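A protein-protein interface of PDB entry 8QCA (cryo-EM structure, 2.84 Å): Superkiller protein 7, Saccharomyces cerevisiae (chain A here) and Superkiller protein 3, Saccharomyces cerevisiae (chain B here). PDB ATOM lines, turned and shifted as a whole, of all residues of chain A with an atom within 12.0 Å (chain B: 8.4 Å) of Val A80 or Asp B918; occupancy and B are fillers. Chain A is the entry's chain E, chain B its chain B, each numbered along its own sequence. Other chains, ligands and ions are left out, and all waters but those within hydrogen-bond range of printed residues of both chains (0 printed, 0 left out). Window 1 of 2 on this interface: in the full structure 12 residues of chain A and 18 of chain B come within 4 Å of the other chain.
Val A80 touches Asp B918.
CD1 of Leu A82 touches O of Val B877, 3.8 Å away.
CD2 of Leu A82 touches O of Asp B878, at 3.98 Å.
O of Asn B919 touches CD1 of Leu A82 (3.6 Å).
Ser A83 touches Ile B922.
Asp B878 touches Lys A85.
Of the printed residues of chain B, Val A80 touches Asp B917, Asp B918 and Asn B919.
Printed residues of chain B within 4 Å of Leu A82: Val B877 (3.8 Å), Asp B878 (3.98 Å) and Asn B919 (3.6 Å).
Of the printed residues of chain B, Ser A83 touches Ile B922 (3.9 Å).
Of the printed residues of chain A, Val B877 touches Leu A82 (3.8 Å).
Of the printed residues of chain A, Asp B878 touches Leu A82 and Lys A85.
Thr B916 touches none of the printed residues of chain A.
Of chain A, only Val A80 comes within 4 Å of Asp B917.
Asp B918 touches just one residue of chain A: Val A80.
Asn B919 touches just these residues of chain A: Val A80, Ser A81 and Leu A82.
No residue of chain A comes within 4 Å of Val B920.
No residue of chain A comes within 4 Å of Ser B921.
Ile B922 touches one residue of chain A.
The nearest residue of chain A that does not touch Asp B918 is Leu A82 (5.7 Å).
The nearest printed residue of chain B that does not touch Leu A82 is Ile B922 (4.2 Å).
OD1 of Asn B919 is in hydrogen-bond range of N of Ser A81 (3.5 Å).
The side-chain amide oxygen of Asn B919 is in hydrogen-bond range of the backbone NH of Val A80 (2.8 Å).
The backbone carbonyl oxygen (O) of Asp B917 sits at hydrogen-bond distance from the backbone NH (N) of Val A80 (3.3 Å).
OG of Ser B921 is in hydrogen-bond range of OD1 of Asp B917.
The side-chain carboxylate of Asp B917 is in salt-bridge range of the side-chain amino group of Lys B925 (3.7 Å).
Of the 10 printed residues of chain A, 5 touch a printed residue of chain B.
Hydrophobic or aromatic side chains of chain A that line the printed part of chain B: Val A80 and Leu A82.
Printed residues of chain B that touch a printed residue of chain A: Val B877, Asp B878, Asp B917, Asp B918, Asn B919 and Ile B922.
Among the printed residues, 9 pairs touch across the chains.
Among the printed residues, no Asp or Glu carboxylate lies within 4 Å of a Lys or Arg side-chain nitrogen of the other chain.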
ATOM      1  N   VAL A  80     -21.556  -7.214  -5.193  1.00  0.00           N
ATOM      2  CA  VAL A  80     -22.929  -7.344  -5.663  1.00  0.00           C
ATOM      3  C   VAL A  80     -23.071  -6.661  -7.019  1.00  0.00           C
ATOM      4  O   VAL A  80     -22.809  -7.265  -8.057  1.00  0.00           O
ATOM      5  CB  VAL A  80     -23.927  -6.762  -4.642  1.00  0.00           C
ATOM      6  CG1 VAL A  80     -25.357  -7.128  -5.018  1.00  0.00           C
ATOM      7  CG2 VAL A  80     -23.596  -7.250  -3.240  1.00  0.00           C
ATOM      8  N   SER A  81     -23.490  -5.393  -7.002  1.00  0.00           N
ATOM      9  CA  SER A  81     -23.640  -4.644  -8.245  1.00  0.00           C
ATOM     10  C   SER A  81     -22.298  -4.439  -8.934  1.00  0.00           C
ATOM     11  O   SER A  81     -22.198  -4.558 -10.160  1.00  0.00           O
ATOM     12  CB  SER A  81     -24.313  -3.301  -7.970  1.00  0.00           C
ATOM     13  OG  SER A  81     -25.584  -3.481  -7.370  1.00  0.00           O
ATOM     14  N   LEU A  82     -21.254  -4.125  -8.164  1.00  0.00           N
ATOM     15  CA  LEU A  82     -19.942  -3.899  -8.760  1.00  0.00           C
ATOM     16  C   LEU A  82     -19.332  -5.199  -9.268  1.00  0.00           C
ATOM     17  O   LEU A  82     -18.590  -5.198 -10.257  1.00  0.00           O
ATOM     18  CB  LEU A  82     -19.015  -3.230  -7.746  1.00  0.00           C
ATOM     19  CG  LEU A  82     -19.398  -1.813  -7.317  1.00  0.00           C
ATOM     20  CD1 LEU A  82     -18.478  -1.323  -6.212  1.00  0.00           C
ATOM     21  CD2 LEU A  82     -19.385  -0.857  -8.498  1.00  0.00           C
ATOM     22  N   SER A  83     -19.627  -6.318  -8.602  1.00  0.00           N
ATOM     23  CA  SER A  83     -19.082  -7.600  -9.035  1.00  0.00           C
ATOM     24  C   SER A  83     -19.755  -8.085 -10.313  1.00  0.00           C
ATOM     25  O   SER A  83     -19.089  -8.620 -11.207  1.00  0.00           O
ATOM     26  CB  SER A  83     -19.231  -8.637  -7.922  1.00  0.00           C
ATOM     27  OG  SER A  83     -18.664  -9.879  -8.299  1.00  0.00           O
ATOM     28  N   LEU A  84     -21.077  -7.917 -10.416  1.00  0.00           N
ATOM     29  CA  LEU A  84     -21.783  -8.333 -11.625  1.00  0.00           C
ATOM     30  C   LEU A  84     -21.326  -7.531 -12.836  1.00  0.00           C
ATOM     31  O   LEU A  84     -21.131  -8.088 -13.922  1.00  0.00           O
ATOM     32  CB  LEU A  84     -23.292  -8.192 -11.430  1.00  0.00           C
ATOM     33  CG  LEU A  84     -23.941  -9.145 -10.427  1.00  0.00           C
ATOM     34  CD1 LEU A  84     -25.420  -8.831 -10.271  1.00  0.00           C
ATOM     35  CD2 LEU A  84     -23.736 -10.591 -10.850  1.00  0.00           C
ATOM     36  N   LYS A  85     -21.156  -6.216 -12.670  1.00  0.00           N
ATOM     37  CA  LYS A  85     -20.682  -5.388 -13.773  1.00  0.00           C
ATOM     38  C   LYS A  85     -19.260  -5.759 -14.170  1.00  0.00           C
ATOM     39  O   LYS A  85     -18.916  -5.743 -15.358  1.00  0.00           O
ATOM     40  CB  LYS A  85     -20.764  -3.910 -13.392  1.00  0.00           C
ATOM     41  CG  LYS A  85     -22.179  -3.395 -13.198  1.00  0.00           C
ATOM     42  CD  LYS A  85     -22.175  -1.944 -12.747  1.00  0.00           C
ATOM     43  CE  LYS A  85     -23.539  -1.523 -12.225  1.00  0.00           C
ATOM     44  NZ  LYS A  85     -23.455  -0.301 -11.377  1.00  0.00           N
ATOM     45  N   LEU A  86     -18.417  -6.085 -13.188  1.00  0.00           N
ATOM     46  CA  LEU A  86     -17.035  -6.446 -13.482  1.00  0.00           C
ATOM     47  C   LEU A  86     -16.959  -7.728 -14.303  1.00  0.00           C
ATOM     48  O   LEU A  86     -16.157  -7.824 -15.240  1.00  0.00           O
ATOM     49  CB  LEU A  86     -16.247  -6.583 -12.179  1.00  0.00           C
ATOM     50  CG  LEU A  86     -14.735  -6.792 -12.255  1.00  0.00           C
ATOM     51  CD1 LEU A  86     -14.046  -6.056 -11.121  1.00  0.00           C
ATOM     52  CD2 LEU A  86     -14.400  -8.271 -12.197  1.00  0.00           C
ATOM     53  N   SER A  87     -17.776  -8.727 -13.962  1.00  0.00           N
ATOM     54  CA  SER A  87     -17.788  -9.967 -14.732  1.00  0.00           C
ATOM     55  C   SER A  87     -18.336  -9.743 -16.136  1.00  0.00           C
ATOM     56  O   SER A  87     -17.798 -10.278 -17.111  1.00  0.00           O
ATOM     57  CB  SER A  87     -18.607 -11.032 -14.000  1.00  0.00           C
ATOM     58  OG  SER A  87     -17.857 -11.621 -12.952  1.00  0.00           O
ATOM     59  N   ALA A  88     -19.409  -8.956 -16.256  1.00  0.00           N
ATOM     60  CA  ALA A  88     -20.004  -8.705 -17.566  1.00  0.00           C
ATOM     61  C   ALA A  88     -19.047  -7.944 -18.474  1.00  0.00           C
ATOM     62  O   ALA A  88     -18.974  -8.214 -19.678  1.00  0.00           O
ATOM     63  CB  ALA A  88     -21.318  -7.941 -17.408  1.00  0.00           C
ATOM     64  N   LEU A  89     -18.311  -6.979 -17.918  1.00  0.00           N
ATOM     65  CA  LEU A  89     -17.367  -6.209 -18.722  1.00  0.00           C
ATOM     66  C   LEU A  89     -16.246  -7.091 -19.259  1.00  0.00           C
ATOM     67  O   LEU A  89     -15.843  -6.955 -20.420  1.00  0.00           O
ATOM     68  CB  LEU A  89     -16.797  -5.055 -17.896  1.00  0.00           C
ATOM     69  CG  LEU A  89     -15.495  -4.435 -18.402  1.00  0.00           C
ATOM     70  CD1 LEU A  89     -15.753  -3.571 -19.626  1.00  0.00           C
ATOM     71  CD2 LEU A  89     -14.825  -3.629 -17.305  1.00  0.00           C
ATOM     72  N   GLU B 874     -20.131   5.830   1.501  1.00  0.00           N
ATOM     73  CA  GLU B 874     -20.452   4.445   1.187  1.00  0.00           C
ATOM     74  C   GLU B 874     -21.870   4.270   0.658  1.00  0.00           C
ATOM     75  O   GLU B 874     -22.145   3.281  -0.030  1.00  0.00           O
ATOM     76  CB  GLU B 874     -20.236   3.576   2.429  1.00  0.00           C
ATOM     77  CG  GLU B 874     -20.419   2.084   2.221  1.00  0.00           C
ATOM     78  CD  GLU B 874     -20.131   1.289   3.477  1.00  0.00           C
ATOM     79  OE1 GLU B 874     -19.668   1.889   4.467  1.00  0.00           O
ATOM     80  OE2 GLU B 874     -20.381   0.065   3.479  1.00  0.00           O
ATOM     81  N   VAL B 877     -21.496   4.130  -3.132  1.00  0.00           N
ATOM     82  CA  VAL B 877     -20.364   3.332  -3.590  1.00  0.00           C
ATOM     83  C   VAL B 877     -20.687   2.554  -4.860  1.00  0.00           C
ATOM     84  O   VAL B 877     -19.769   2.172  -5.595  1.00  0.00           O
ATOM     85  CB  VAL B 877     -19.894   2.380  -2.475  1.00  0.00           C
ATOM     86  CG1 VAL B 877     -20.897   1.259  -2.264  1.00  0.00           C
ATOM     87  CG2 VAL B 877     -18.508   1.828  -2.775  1.00  0.00           C
ATOM     88  N   ASP B 878     -21.970   2.325  -5.152  1.00  0.00           N
ATOM     89  CA  ASP B 878     -22.354   1.592  -6.352  1.00  0.00           C
ATOM     90  C   ASP B 878     -22.157   2.400  -7.626  1.00  0.00           C
ATOM     91  O   ASP B 878     -22.304   1.844  -8.719  1.00  0.00           O
ATOM     92  CB  ASP B 878     -23.811   1.143  -6.248  1.00  0.00           C
ATOM     93  CG  ASP B 878     -24.741   2.269  -5.844  1.00  0.00           C
ATOM     94  OD1 ASP B 878     -24.751   2.637  -4.652  1.00  0.00           O
ATOM     95  OD2 ASP B 878     -25.466   2.786  -6.720  1.00  0.00           O
ATOM     96  N   SER B 914     -13.018 -13.070  -9.463  1.00  0.00           N
ATOM     97  CA  SER B 914     -13.449 -13.087  -8.074  1.00  0.00           C
ATOM     98  C   SER B 914     -14.961 -13.244  -8.008  1.00  0.00           C
ATOM     99  O   SER B 914     -15.684 -12.916  -8.951  1.00  0.00           O
ATOM    100  CB  SER B 914     -13.019 -11.812  -7.335  1.00  0.00           C
ATOM    101  N   THR B 915     -15.433 -13.756  -6.872  1.00  0.00           N
ATOM    102  CA  THR B 915     -16.855 -13.977  -6.662  1.00  0.00           C
ATOM    103  C   THR B 915     -17.165 -13.835  -5.179  1.00  0.00           C
ATOM    104  O   THR B 915     -16.273 -13.901  -4.330  1.00  0.00           O
ATOM    105  CB  THR B 915     -17.300 -15.354  -7.169  1.00  0.00           C
ATOM    106  OG1 THR B 915     -18.723 -15.472  -7.052  1.00  0.00           O
ATOM    107  CG2 THR B 915     -16.636 -16.460  -6.361  1.00  0.00           C
ATOM    108  N   THR B 916     -18.453 -13.640  -4.883  1.00  0.00           N
ATOM    109  CA  THR B 916     -18.935 -13.464  -3.511  1.00  0.00           C
ATOM    110  C   THR B 916     -18.196 -12.329  -2.807  1.00  0.00           C
ATOM    111  O   THR B 916     -17.826 -12.434  -1.637  1.00  0.00           O
ATOM    112  CB  THR B 916     -18.823 -14.763  -2.709  1.00  0.00           C
ATOM    113  N   ASP B 917     -17.978 -11.233  -3.530  1.00  0.00           N
ATOM    114  CA  ASP B 917     -17.229 -10.090  -3.031  1.00  0.00           C
ATOM    115  C   ASP B 917     -18.151  -8.882  -2.961  1.00  0.00           C
ATOM    116  O   ASP B 917     -18.882  -8.600  -3.917  1.00  0.00           O
ATOM    117  CB  ASP B 917     -16.025  -9.793  -3.929  1.00  0.00           C
ATOM    118  CG  ASP B 917     -14.931  -9.042  -3.203  1.00  0.00           C
ATOM    119  OD1 ASP B 917     -15.086  -8.803  -1.990  1.00  0.00           O
ATOM    120  OD2 ASP B 917     -13.918  -8.695  -3.844  1.00  0.00           O
ATOM    121  N   ASP B 918     -18.116  -8.175  -1.836  1.00  0.00           N
ATOM    122  CA  ASP B 918     -18.995  -7.036  -1.628  1.00  0.00           C
ATOM    123  C   ASP B 918     -18.475  -5.807  -2.372  1.00  0.00           C
ATOM    124  O   ASP B 918     -17.329  -5.752  -2.822  1.00  0.00           O
ATOM    125  CB  ASP B 918     -19.137  -6.736  -0.137  1.00  0.00           C
ATOM    126  CG  ASP B 918     -20.514  -6.222   0.224  1.00  0.00           C
ATOM    127  OD1 ASP B 918     -20.630  -5.472   1.217  1.00  0.00           O
ATOM    128  OD2 ASP B 918     -21.484  -6.563  -0.486  1.00  0.00           O
ATOM    129  N   ASN B 919     -19.351  -4.806  -2.498  1.00  0.00           N
ATOM    130  CA  ASN B 919     -18.988  -3.581  -3.202  1.00  0.00           C
ATOM    131  C   ASN B 919     -17.863  -2.839  -2.488  1.00  0.00           C
ATOM    132  O   ASN B 919     -16.934  -2.337  -3.131  1.00  0.00           O
ATOM    133  CB  ASN B 919     -20.215  -2.679  -3.340  1.00  0.00           C
ATOM    134  CG  ASN B 919     -21.283  -3.279  -4.231  1.00  0.00           C
ATOM    135  OD1 ASN B 919     -21.272  -4.476  -4.513  1.00  0.00           O
ATOM    136  ND2 ASN B 919     -22.215  -2.447  -4.677  1.00  0.00           N
ATOM    137  N   VAL B 920     -17.935  -2.757  -1.158  1.00  0.00           N
ATOM    138  CA  VAL B 920     -16.944  -1.999  -0.401  1.00  0.00           C
ATOM    139  C   VAL B 920     -15.585  -2.685  -0.453  1.00  0.00           C
ATOM    140  O   VAL B 920     -14.541  -2.022  -0.500  1.00  0.00           O
ATOM    141  CB  VAL B 920     -17.424  -1.798   1.047  1.00  0.00           C
ATOM    142  CG1 VAL B 920     -16.509  -0.829   1.781  1.00  0.00           C
ATOM    143  CG2 VAL B 920     -18.859  -1.304   1.057  1.00  0.00           C
ATOM    144  N   SER B 921     -15.572  -4.019  -0.434  1.00  0.00           N
ATOM    145  CA  SER B 921     -14.310  -4.741  -0.554  1.00  0.00           C
ATOM    146  C   SER B 921     -13.655  -4.484  -1.905  1.00  0.00           C
ATOM    147  O   SER B 921     -12.437  -4.284  -1.986  1.00  0.00           O
ATOM    148  CB  SER B 921     -14.541  -6.234  -0.340  1.00  0.00           C
ATOM    149  OG  SER B 921     -13.428  -6.991  -0.779  1.00  0.00           O
ATOM    150  N   ILE B 922     -14.446  -4.481  -2.979  1.00  0.00           N
ATOM    151  CA  ILE B 922     -13.908  -4.166  -4.298  1.00  0.00           C
ATOM    152  C   ILE B 922     -13.410  -2.728  -4.342  1.00  0.00           C
ATOM    153  O   ILE B 922     -12.383  -2.432  -4.961  1.00  0.00           O
ATOM    154  CB  ILE B 922     -14.962  -4.438  -5.387  1.00  0.00           C
ATOM    155  CG1 ILE B 922     -15.385  -5.907  -5.364  1.00  0.00           C
ATOM    156  CG2 ILE B 922     -14.427  -4.068  -6.758  1.00  0.00           C
ATOM    157  CD1 ILE B 922     -16.429  -6.256  -6.395  1.00  0.00           C
ATOM    158  N   ALA B 923     -14.126  -1.811  -3.687  1.00  0.00           N
ATOM    159  CA  ALA B 923     -13.679  -0.421  -3.635  1.00  0.00           C
ATOM    160  C   ALA B 923     -12.327  -0.305  -2.941  1.00  0.00           C
ATOM    161  O   ALA B 923     -11.432   0.407  -3.413  1.00  0.00           O
ATOM    162  CB  ALA B 923     -14.727   0.437  -2.926  1.00  0.00           C
ATOM    163  N   CYS B 924     -12.155  -1.010  -1.822  1.00  0.00           N
ATOM    164  CA  CYS B 924     -10.886  -0.954  -1.099  1.00  0.00           C
ATOM    165  C   CYS B 924      -9.764  -1.625  -1.884  1.00  0.00           C
ATOM    166  O   CYS B 924      -8.612  -1.174  -1.844  1.00  0.00           O
ATOM    167  CB  CYS B 924     -11.039  -1.597   0.278  1.00  0.00           C
ATOM    168  SG  CYS B 924     -12.187  -0.740   1.380  1.00  0.00           S
ATOM    169  N   LYS B 925     -10.075  -2.704  -2.603  1.00  0.00           N
ATOM    170  CA  LYS B 925      -9.054  -3.354  -3.420  1.00  0.00           C
ATOM    171  C   LYS B 925      -8.644  -2.472  -4.594  1.00  0.00           C
ATOM    172  O   LYS B 925      -7.474  -2.458  -4.990  1.00  0.00           O
ATOM    173  CB  LYS B 925      -9.555  -4.713  -3.903  1.00  0.00           C
ATOM    174  CG  LYS B 925      -9.330  -5.833  -2.902  1.00  0.00           C
ATOM    175  CD  LYS B 925      -9.808  -7.170  -3.437  1.00  0.00           C
ATOM    176  CE  LYS B 925     -10.117  -8.138  -2.310  1.00  0.00           C
ATOM    177  NZ  LYS B 925     -10.433  -9.501  -2.818  1.00  0.00           N
ATOM    178  N   LEU B 966     -12.268  -3.284   6.564  1.00  0.00           N
ATOM    179  CA  LEU B 966     -12.686  -4.667   6.376  1.00  0.00           C
ATOM    180  C   LEU B 966     -12.299  -5.602   7.513  1.00  0.00           C
ATOM    181  O   LEU B 966     -12.886  -6.683   7.619  1.00  0.00           O
ATOM    182  CB  LEU B 966     -12.108  -5.221   5.066  1.00  0.00           C
ATOM    183  CG  LEU B 966     -12.468  -4.443   3.802  1.00  0.00           C
ATOM    184  CD1 LEU B 966     -11.842  -5.089   2.576  1.00  0.00           C
ATOM    185  CD2 LEU B 966     -13.976  -4.334   3.648  1.00  0.00           C
ATOM    186  N   ASP B1138     -26.503   1.064   6.728  1.00  0.00           N
ATOM    187  CA  ASP B1138     -26.582  -0.352   7.092  1.00  0.00           C
ATOM    188  C   ASP B1138     -25.983  -0.628   8.470  1.00  0.00           C
ATOM    189  O   ASP B1138     -25.436  -1.705   8.714  1.00  0.00           O
ATOM    190  CB  ASP B1138     -25.914  -1.238   6.036  1.00  0.00           C
ATOM    191  CG  ASP B1138     -26.703  -1.300   4.744  1.00  0.00           C
ATOM    192  OD1 ASP B1138     -27.839  -0.783   4.716  1.00  0.00           O
ATOM    193  OD2 ASP B1138     -26.187  -1.865   3.759  1.00  0.00           O
